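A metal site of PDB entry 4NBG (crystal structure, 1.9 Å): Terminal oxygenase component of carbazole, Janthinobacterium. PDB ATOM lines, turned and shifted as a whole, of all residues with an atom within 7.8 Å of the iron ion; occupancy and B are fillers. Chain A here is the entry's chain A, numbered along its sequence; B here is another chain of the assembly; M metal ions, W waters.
The side-chain carboxylate (OD1) of Asp 333 sits close to the side-chain amide nitrogen (ND2) of Asn 177, at 2.9 Å. The side-chain amide nitrogen (ND2) of Asn 330 lies within hydrogen-bond range of the side-chain carboxylate (OD2) of Asp 333 (2.9 Å). O of Asp 333 lies close to NE of Arg 337 (3.3 Å). A ring nitrogen (ND1) of His 183 lies within hydrogen-bond range of the backbone carbonyl oxygen of Asn 177, at 3.0 Å. ND1 of His 183 sits at hydrogen-bond distance from O of Asp 180, at 2.6 Å. ND1 of His 187 lies close to O of Phe 329 (3.3 Å).
The iron ion is bound by water W1 (1.9 Å), the side-chain carboxylate (OD1) of Asp 333 (2.0 Å), a ring nitrogen (NE2) of His 183 (2.0 Å) and a ring nitrogen (NE2) of His 187 (2.1 Å). The iron ion has four donor atoms within binding distance. Slightly farther from the iron ion lies OD2 of Asp 333 (2.6 Å).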
ATOM      1  N   ASN A 177     -24.180   7.546   2.163  1.00  0.00           N
ATOM      2  CA  ASN A 177     -24.999   6.400   1.799  1.00  0.00           C
ATOM      3  C   ASN A 177     -24.526   5.166   2.572  1.00  0.00           C
ATOM      4  O   ASN A 177     -25.336   4.401   3.094  1.00  0.00           O
ATOM      5  CB  ASN A 177     -24.907   6.109   0.305  1.00  0.00           C
ATOM      6  CG  ASN A 177     -25.617   4.829  -0.071  1.00  0.00           C
ATOM      7  OD1 ASN A 177     -26.853   4.767  -0.082  1.00  0.00           O
ATOM      8  ND2 ASN A 177     -24.853   3.781  -0.355  1.00  0.00           N
ATOM      9  N   GLY A 178     -23.215   4.980   2.650  1.00  0.00           N
ATOM     10  CA  GLY A 178     -22.693   3.819   3.358  1.00  0.00           C
ATOM     11  C   GLY A 178     -23.014   3.750   4.839  1.00  0.00           C
ATOM     12  O   GLY A 178     -23.271   2.666   5.377  1.00  0.00           O
ATOM     13  N   PHE A 179     -23.021   4.903   5.495  1.00  0.00           N
ATOM     14  CA  PHE A 179     -23.273   4.969   6.940  1.00  0.00           C
ATOM     15  C   PHE A 179     -24.766   5.201   7.265  1.00  0.00           C
ATOM     16  O   PHE A 179     -25.155   5.233   8.438  1.00  0.00           O
ATOM     17  CB  PHE A 179     -22.431   6.103   7.526  1.00  0.00           C
ATOM     18  CG  PHE A 179     -22.377   6.109   9.031  1.00  0.00           C
ATOM     19  CD1 PHE A 179     -21.978   4.976   9.733  1.00  0.00           C
ATOM     20  CD2 PHE A 179     -22.696   7.264   9.745  1.00  0.00           C
ATOM     21  CE1 PHE A 179     -21.899   4.985  11.133  1.00  0.00           C
ATOM     22  CE2 PHE A 179     -22.617   7.288  11.133  1.00  0.00           C
ATOM     23  CZ  PHE A 179     -22.214   6.142  11.835  1.00  0.00           C
ATOM     24  N   ASP A 180     -25.571   5.335   6.220  1.00  0.00           N
ATOM     25  CA  ASP A 180     -27.021   5.574   6.321  1.00  0.00           C
ATOM     26  C   ASP A 180     -27.745   4.333   6.872  1.00  0.00           C
ATOM     27  O   ASP A 180     -27.883   3.337   6.159  1.00  0.00           O
ATOM     28  CB  ASP A 180     -27.544   5.917   4.921  1.00  0.00           C
ATOM     29  CG  ASP A 180     -28.962   6.451   4.927  1.00  0.00           C
ATOM     30  OD1 ASP A 180     -29.788   6.016   5.754  1.00  0.00           O
ATOM     31  OD2 ASP A 180     -29.246   7.313   4.063  1.00  0.00           O
ATOM     32  N   HIS A 183     -30.727   3.160   4.647  1.00  0.00           N
ATOM     33  CA  HIS A 183     -30.517   2.849   3.233  1.00  0.00           C
ATOM     34  C   HIS A 183     -30.552   1.339   2.990  1.00  0.00           C
ATOM     35  O   HIS A 183     -30.610   0.893   1.848  1.00  0.00           O
ATOM     36  CB  HIS A 183     -29.196   3.452   2.710  1.00  0.00           C
ATOM     37  CG  HIS A 183     -28.032   2.521   2.754  1.00  0.00           C
ATOM     38  ND1 HIS A 183     -27.314   2.272   3.907  1.00  0.00           N
ATOM     39  CD2 HIS A 183     -27.446   1.776   1.786  1.00  0.00           C
ATOM     40  CE1 HIS A 183     -26.340   1.419   3.638  1.00  0.00           C
ATOM     41  NE2 HIS A 183     -26.401   1.095   2.361  1.00  0.00           N
ATOM     42  N   ILE A 184     -30.540   0.583   4.072  1.00  0.00           N
ATOM     43  CA  ILE A 184     -30.599  -0.870   4.022  1.00  0.00           C
ATOM     44  C   ILE A 184     -31.774  -1.327   3.146  1.00  0.00           C
ATOM     45  O   ILE A 184     -31.773  -2.428   2.598  1.00  0.00           O
ATOM     46  CB  ILE A 184     -30.759  -1.443   5.454  1.00  0.00           C
ATOM     47  CG1 ILE A 184     -30.566  -2.947   5.455  1.00  0.00           C
ATOM     48  CG2 ILE A 184     -32.131  -1.085   6.005  1.00  0.00           C
ATOM     49  CD1 ILE A 184     -30.520  -3.529   6.861  1.00  0.00           C
ATOM     50  N   TYR A 185     -32.762  -0.450   3.001  1.00  0.00           N
ATOM     51  CA  TYR A 185     -33.939  -0.742   2.182  1.00  0.00           C
ATOM     52  C   TYR A 185     -33.576  -1.079   0.716  1.00  0.00           C
ATOM     53  O   TYR A 185     -34.223  -1.917   0.094  1.00  0.00           O
ATOM     54  CB  TYR A 185     -34.904   0.445   2.210  1.00  0.00           C
ATOM     55  CG  TYR A 185     -36.216   0.225   1.484  1.00  0.00           C
ATOM     56  CD1 TYR A 185     -37.201  -0.597   2.019  1.00  0.00           C
ATOM     57  CD2 TYR A 185     -36.456   0.831   0.251  1.00  0.00           C
ATOM     58  CE1 TYR A 185     -38.411  -0.818   1.347  1.00  0.00           C
ATOM     59  CE2 TYR A 185     -37.663   0.612  -0.434  1.00  0.00           C
ATOM     60  CZ  TYR A 185     -38.633  -0.207   0.120  1.00  0.00           C
ATOM     61  OH  TYR A 185     -39.808  -0.426  -0.563  1.00  0.00           O
ATOM     62  N   ILE A 186     -32.543  -0.428   0.183  1.00  0.00           N
ATOM     63  CA  ILE A 186     -32.142  -0.665  -1.206  1.00  0.00           C
ATOM     64  C   ILE A 186     -31.526  -2.051  -1.407  1.00  0.00           C
ATOM     65  O   ILE A 186     -31.370  -2.504  -2.542  1.00  0.00           O
ATOM     66  CB  ILE A 186     -31.124   0.383  -1.732  1.00  0.00           C
ATOM     67  CG1 ILE A 186     -29.750   0.164  -1.092  1.00  0.00           C
ATOM     68  CG2 ILE A 186     -31.641   1.789  -1.452  1.00  0.00           C
ATOM     69  CD1 ILE A 186     -28.652   1.066  -1.663  1.00  0.00           C
ATOM     70  N   HIS A 187     -31.174  -2.711  -0.309  1.00  0.00           N
ATOM     71  CA  HIS A 187     -30.557  -4.024  -0.374  1.00  0.00           C
ATOM     72  C   HIS A 187     -31.519  -5.195  -0.182  1.00  0.00           C
ATOM     73  O   HIS A 187     -31.106  -6.341  -0.171  1.00  0.00           O
ATOM     74  CB  HIS A 187     -29.462  -4.134   0.691  1.00  0.00           C
ATOM     75  CG  HIS A 187     -28.302  -3.212   0.463  1.00  0.00           C
ATOM     76  ND1 HIS A 187     -27.540  -3.250  -0.690  1.00  0.00           N
ATOM     77  CD2 HIS A 187     -27.790  -2.216   1.219  1.00  0.00           C
ATOM     78  CE1 HIS A 187     -26.604  -2.317  -0.621  1.00  0.00           C
ATOM     79  NE2 HIS A 187     -26.731  -1.675   0.524  1.00  0.00           N
ATOM     80  N   LEU A 270     -15.592   3.218   5.882  1.00  0.00           N
ATOM     81  CA  LEU A 270     -16.605   2.509   6.646  1.00  0.00           C
ATOM     82  C   LEU A 270     -16.158   1.113   7.033  1.00  0.00           C
ATOM     83  O   LEU A 270     -15.486   0.416   6.255  1.00  0.00           O
ATOM     84  CB  LEU A 270     -17.892   2.403   5.807  1.00  0.00           C
ATOM     85  CG  LEU A 270     -19.157   1.878   6.492  1.00  0.00           C
ATOM     86  CD1 LEU A 270     -19.827   3.004   7.271  1.00  0.00           C
ATOM     87  CD2 LEU A 270     -20.124   1.333   5.446  1.00  0.00           C
ATOM     88  N   PHE A 275     -19.075  -8.967   8.240  1.00  0.00           N
ATOM     89  CA  PHE A 275     -19.712  -8.874   6.922  1.00  0.00           C
ATOM     90  C   PHE A 275     -18.762  -9.410   5.857  1.00  0.00           C
ATOM     91  O   PHE A 275     -17.554  -9.176   5.932  1.00  0.00           O
ATOM     92  CB  PHE A 275     -20.053  -7.412   6.622  1.00  0.00           C
ATOM     93  CG  PHE A 275     -21.046  -7.246   5.507  1.00  0.00           C
ATOM     94  CD1 PHE A 275     -22.406  -7.415   5.736  1.00  0.00           C
ATOM     95  CD2 PHE A 275     -20.625  -6.916   4.225  1.00  0.00           C
ATOM     96  CE1 PHE A 275     -23.327  -7.272   4.707  1.00  0.00           C
ATOM     97  CE2 PHE A 275     -21.545  -6.758   3.185  1.00  0.00           C
ATOM     98  CZ  PHE A 275     -22.896  -6.940   3.429  1.00  0.00           C
ATOM     99  N   GLU A 284     -14.559  -0.235   3.540  1.00  0.00           N
ATOM    100  CA  GLU A 284     -14.600   0.408   2.240  1.00  0.00           C
ATOM    101  C   GLU A 284     -14.333   1.908   2.346  1.00  0.00           C
ATOM    102  O   GLU A 284     -14.908   2.603   3.192  1.00  0.00           O
ATOM    103  CB  GLU A 284     -15.935   0.159   1.540  1.00  0.00           C
ATOM    104  CG  GLU A 284     -17.184   0.506   2.338  1.00  0.00           C
ATOM    105  CD  GLU A 284     -18.457   0.401   1.519  1.00  0.00           C
ATOM    106  OE1 GLU A 284     -18.543  -0.509   0.661  1.00  0.00           O
ATOM    107  OE2 GLU A 284     -19.378   1.204   1.730  1.00  0.00           O
ATOM    108  N   TYR A 286     -13.996   5.761   0.355  1.00  0.00           N
ATOM    109  CA  TYR A 286     -14.606   6.554  -0.710  1.00  0.00           C
ATOM    110  C   TYR A 286     -13.591   7.692  -0.846  1.00  0.00           C
ATOM    111  O   TYR A 286     -13.688   8.727  -0.165  1.00  0.00           O
ATOM    112  CB  TYR A 286     -15.973   7.101  -0.261  1.00  0.00           C
ATOM    113  CG  TYR A 286     -16.778   6.091   0.531  1.00  0.00           C
ATOM    114  CD1 TYR A 286     -17.478   5.067  -0.102  1.00  0.00           C
ATOM    115  CD2 TYR A 286     -16.842   6.176   1.918  1.00  0.00           C
ATOM    116  CE1 TYR A 286     -18.232   4.136   0.650  1.00  0.00           C
ATOM    117  CE2 TYR A 286     -17.580   5.272   2.670  1.00  0.00           C
ATOM    118  CZ  TYR A 286     -18.271   4.257   2.034  1.00  0.00           C
ATOM    119  OH  TYR A 286     -19.014   3.394   2.804  1.00  0.00           O
ATOM    120  N   TYR A 296     -13.816   3.833  -5.235  1.00  0.00           N
ATOM    121  CA  TYR A 296     -14.627   3.020  -4.330  1.00  0.00           C
ATOM    122  C   TYR A 296     -13.700   1.852  -4.040  1.00  0.00           C
ATOM    123  O   TYR A 296     -13.672   0.861  -4.767  1.00  0.00           O
ATOM    124  CB  TYR A 296     -15.918   2.564  -5.027  1.00  0.00           C
ATOM    125  CG  TYR A 296     -16.831   1.720  -4.151  1.00  0.00           C
ATOM    126  CD1 TYR A 296     -16.867   1.878  -2.769  1.00  0.00           C
ATOM    127  CD2 TYR A 296     -17.701   0.791  -4.729  1.00  0.00           C
ATOM    128  CE1 TYR A 296     -17.739   1.129  -1.980  1.00  0.00           C
ATOM    129  CE2 TYR A 296     -18.578   0.041  -3.957  1.00  0.00           C
ATOM    130  CZ  TYR A 296     -18.585   0.220  -2.578  1.00  0.00           C
ATOM    131  OH  TYR A 296     -19.456  -0.513  -1.802  1.00  0.00           O
ATOM    132  N   PHE A 329     -23.934  -7.180  -3.637  1.00  0.00           N
ATOM    133  CA  PHE A 329     -24.585  -6.396  -2.595  1.00  0.00           C
ATOM    134  C   PHE A 329     -24.346  -4.910  -2.806  1.00  0.00           C
ATOM    135  O   PHE A 329     -25.296  -4.121  -2.881  1.00  0.00           O
ATOM    136  CB  PHE A 329     -24.065  -6.819  -1.228  1.00  0.00           C
ATOM    137  CG  PHE A 329     -24.788  -6.182  -0.071  1.00  0.00           C
ATOM    138  CD1 PHE A 329     -25.976  -6.737   0.410  1.00  0.00           C
ATOM    139  CD2 PHE A 329     -24.273  -5.055   0.561  1.00  0.00           C
ATOM    140  CE1 PHE A 329     -26.631  -6.168   1.506  1.00  0.00           C
ATOM    141  CE2 PHE A 329     -24.919  -4.484   1.659  1.00  0.00           C
ATOM    142  CZ  PHE A 329     -26.102  -5.038   2.127  1.00  0.00           C
ATOM    143  N   ASN A 330     -23.082  -4.521  -2.932  1.00  0.00           N
ATOM    144  CA  ASN A 330     -22.727  -3.111  -3.085  1.00  0.00           C
ATOM    145  C   ASN A 330     -23.017  -2.425  -4.414  1.00  0.00           C
ATOM    146  O   ASN A 330     -22.994  -1.200  -4.486  1.00  0.00           O
ATOM    147  CB  ASN A 330     -21.252  -2.899  -2.734  1.00  0.00           C
ATOM    148  CG  ASN A 330     -20.953  -3.262  -1.295  1.00  0.00           C
ATOM    149  OD1 ASN A 330     -20.096  -4.097  -1.016  1.00  0.00           O
ATOM    150  ND2 ASN A 330     -21.656  -2.616  -0.362  1.00  0.00           N
ATOM    151  N   ASN A 331     -23.283  -3.172  -5.480  1.00  0.00           N
ATOM    152  CA  ASN A 331     -23.568  -2.502  -6.749  1.00  0.00           C
ATOM    153  C   ASN A 331     -24.767  -1.565  -6.601  1.00  0.00           C
ATOM    154  O   ASN A 331     -24.837  -0.531  -7.257  1.00  0.00           O
ATOM    155  CB  ASN A 331     -23.819  -3.519  -7.873  1.00  0.00           C
ATOM    156  CG  ASN A 331     -22.524  -4.016  -8.489  1.00  0.00           C
ATOM    157  OD1 ASN A 331     -21.440  -3.533  -8.152  1.00  0.00           O
ATOM    158  ND2 ASN A 331     -22.626  -4.994  -9.382  1.00  0.00           N
ATOM    159  N   ASP A 332     -25.718  -1.901  -5.726  1.00  0.00           N
ATOM    160  CA  ASP A 332     -26.873  -1.036  -5.536  1.00  0.00           C
ATOM    161  C   ASP A 332     -26.452   0.268  -4.838  1.00  0.00           C
ATOM    162  O   ASP A 332     -27.109   1.298  -5.008  1.00  0.00           O
ATOM    163  CB  ASP A 332     -27.969  -1.730  -4.730  1.00  0.00           C
ATOM    164  CG  ASP A 332     -28.698  -2.775  -5.546  1.00  0.00           C
ATOM    165  OD1 ASP A 332     -29.011  -2.509  -6.725  1.00  0.00           O
ATOM    166  OD2 ASP A 332     -28.974  -3.872  -5.008  1.00  0.00           O
ATOM    167  N   ASP A 333     -25.382   0.232  -4.063  1.00  0.00           N
ATOM    168  CA  ASP A 333     -24.899   1.428  -3.381  1.00  0.00           C
ATOM    169  C   ASP A 333     -24.338   2.398  -4.412  1.00  0.00           C
ATOM    170  O   ASP A 333     -24.417   3.616  -4.248  1.00  0.00           O
ATOM    171  CB  ASP A 333     -23.807   1.087  -2.375  1.00  0.00           C
ATOM    172  CG  ASP A 333     -24.335   0.342  -1.178  1.00  0.00           C
ATOM    173  OD1 ASP A 333     -25.238   0.879  -0.502  1.00  0.00           O
ATOM    174  OD2 ASP A 333     -23.862  -0.781  -0.914  1.00  0.00           O
ATOM    175  N   ILE A 334     -23.762   1.845  -5.478  1.00  0.00           N
ATOM    176  CA  ILE A 334     -23.187   2.674  -6.523  1.00  0.00           C
ATOM    177  C   ILE A 334     -24.233   3.542  -7.217  1.00  0.00           C
ATOM    178  O   ILE A 334     -24.067   4.764  -7.296  1.00  0.00           O
ATOM    179  CB  ILE A 334     -22.458   1.808  -7.580  1.00  0.00           C
ATOM    180  CG1 ILE A 334     -21.208   1.188  -6.947  1.00  0.00           C
ATOM    181  CG2 ILE A 334     -22.075   2.650  -8.795  1.00  0.00           C
ATOM    182  CD1 ILE A 334     -20.472   0.192  -7.846  1.00  0.00           C
ATOM    183  N   ALA A 336     -27.155   4.266  -6.102  1.00  0.00           N
ATOM    184  CA  ALA A 336     -27.852   5.047  -5.083  1.00  0.00           C
ATOM    185  C   ALA A 336     -27.099   6.368  -4.890  1.00  0.00           C
ATOM    186  O   ALA A 336     -27.702   7.437  -4.836  1.00  0.00           O
ATOM    187  CB  ALA A 336     -27.920   4.275  -3.759  1.00  0.00           C
ATOM    188  N   ARG A 337     -25.779   6.286  -4.781  1.00  0.00           N
ATOM    189  CA  ARG A 337     -24.939   7.484  -4.635  1.00  0.00           C
ATOM    190  C   ARG A 337     -25.133   8.397  -5.823  1.00  0.00           C
ATOM    191  O   ARG A 337     -25.280   9.607  -5.675  1.00  0.00           O
ATOM    192  CB  ARG A 337     -23.460   7.131  -4.622  1.00  0.00           C
ATOM    193  CG  ARG A 337     -23.025   6.236  -3.549  1.00  0.00           C
ATOM    194  CD  ARG A 337     -21.635   5.747  -3.850  1.00  0.00           C
ATOM    195  NE  ARG A 337     -21.456   4.504  -3.156  1.00  0.00           N
ATOM    196  CZ  ARG A 337     -20.384   3.737  -3.233  1.00  0.00           C
ATOM    197  NH1 ARG A 337     -19.348   4.087  -3.989  1.00  0.00           N
ATOM    198  NH2 ARG A 337     -20.358   2.604  -2.544  1.00  0.00           N
ATOM    199  N   TYR B  92     -35.296   4.606  -2.229  1.00  0.00           N
ATOM    200  CA  TYR B  92     -34.158   4.791  -1.323  1.00  0.00           C
ATOM    201  C   TYR B  92     -34.433   4.436   0.144  1.00  0.00           C
ATOM    202  O   TYR B  92     -33.877   3.466   0.663  1.00  0.00           O
ATOM    203  CB  TYR B  92     -33.638   6.231  -1.442  1.00  0.00           C
ATOM    204  CG  TYR B  92     -32.150   6.423  -1.209  1.00  0.00           C
ATOM    205  CD1 TYR B  92     -31.355   5.407  -0.665  1.00  0.00           C
ATOM    206  CD2 TYR B  92     -31.539   7.658  -1.460  1.00  0.00           C
ATOM    207  CE1 TYR B  92     -29.999   5.616  -0.375  1.00  0.00           C
ATOM    208  CE2 TYR B  92     -30.192   7.872  -1.178  1.00  0.00           C
ATOM    209  CZ  TYR B  92     -29.428   6.857  -0.637  1.00  0.00           C
ATOM    210  OH  TYR B  92     -28.095   7.110  -0.341  1.00  0.00           O
HETATM  211 FE    FE M   1     -25.413  -0.203   1.146  1.00  0.00          FE
HETATM  212  O   HOH W   1     -23.721  -0.375   1.929  1.00  0.00           O
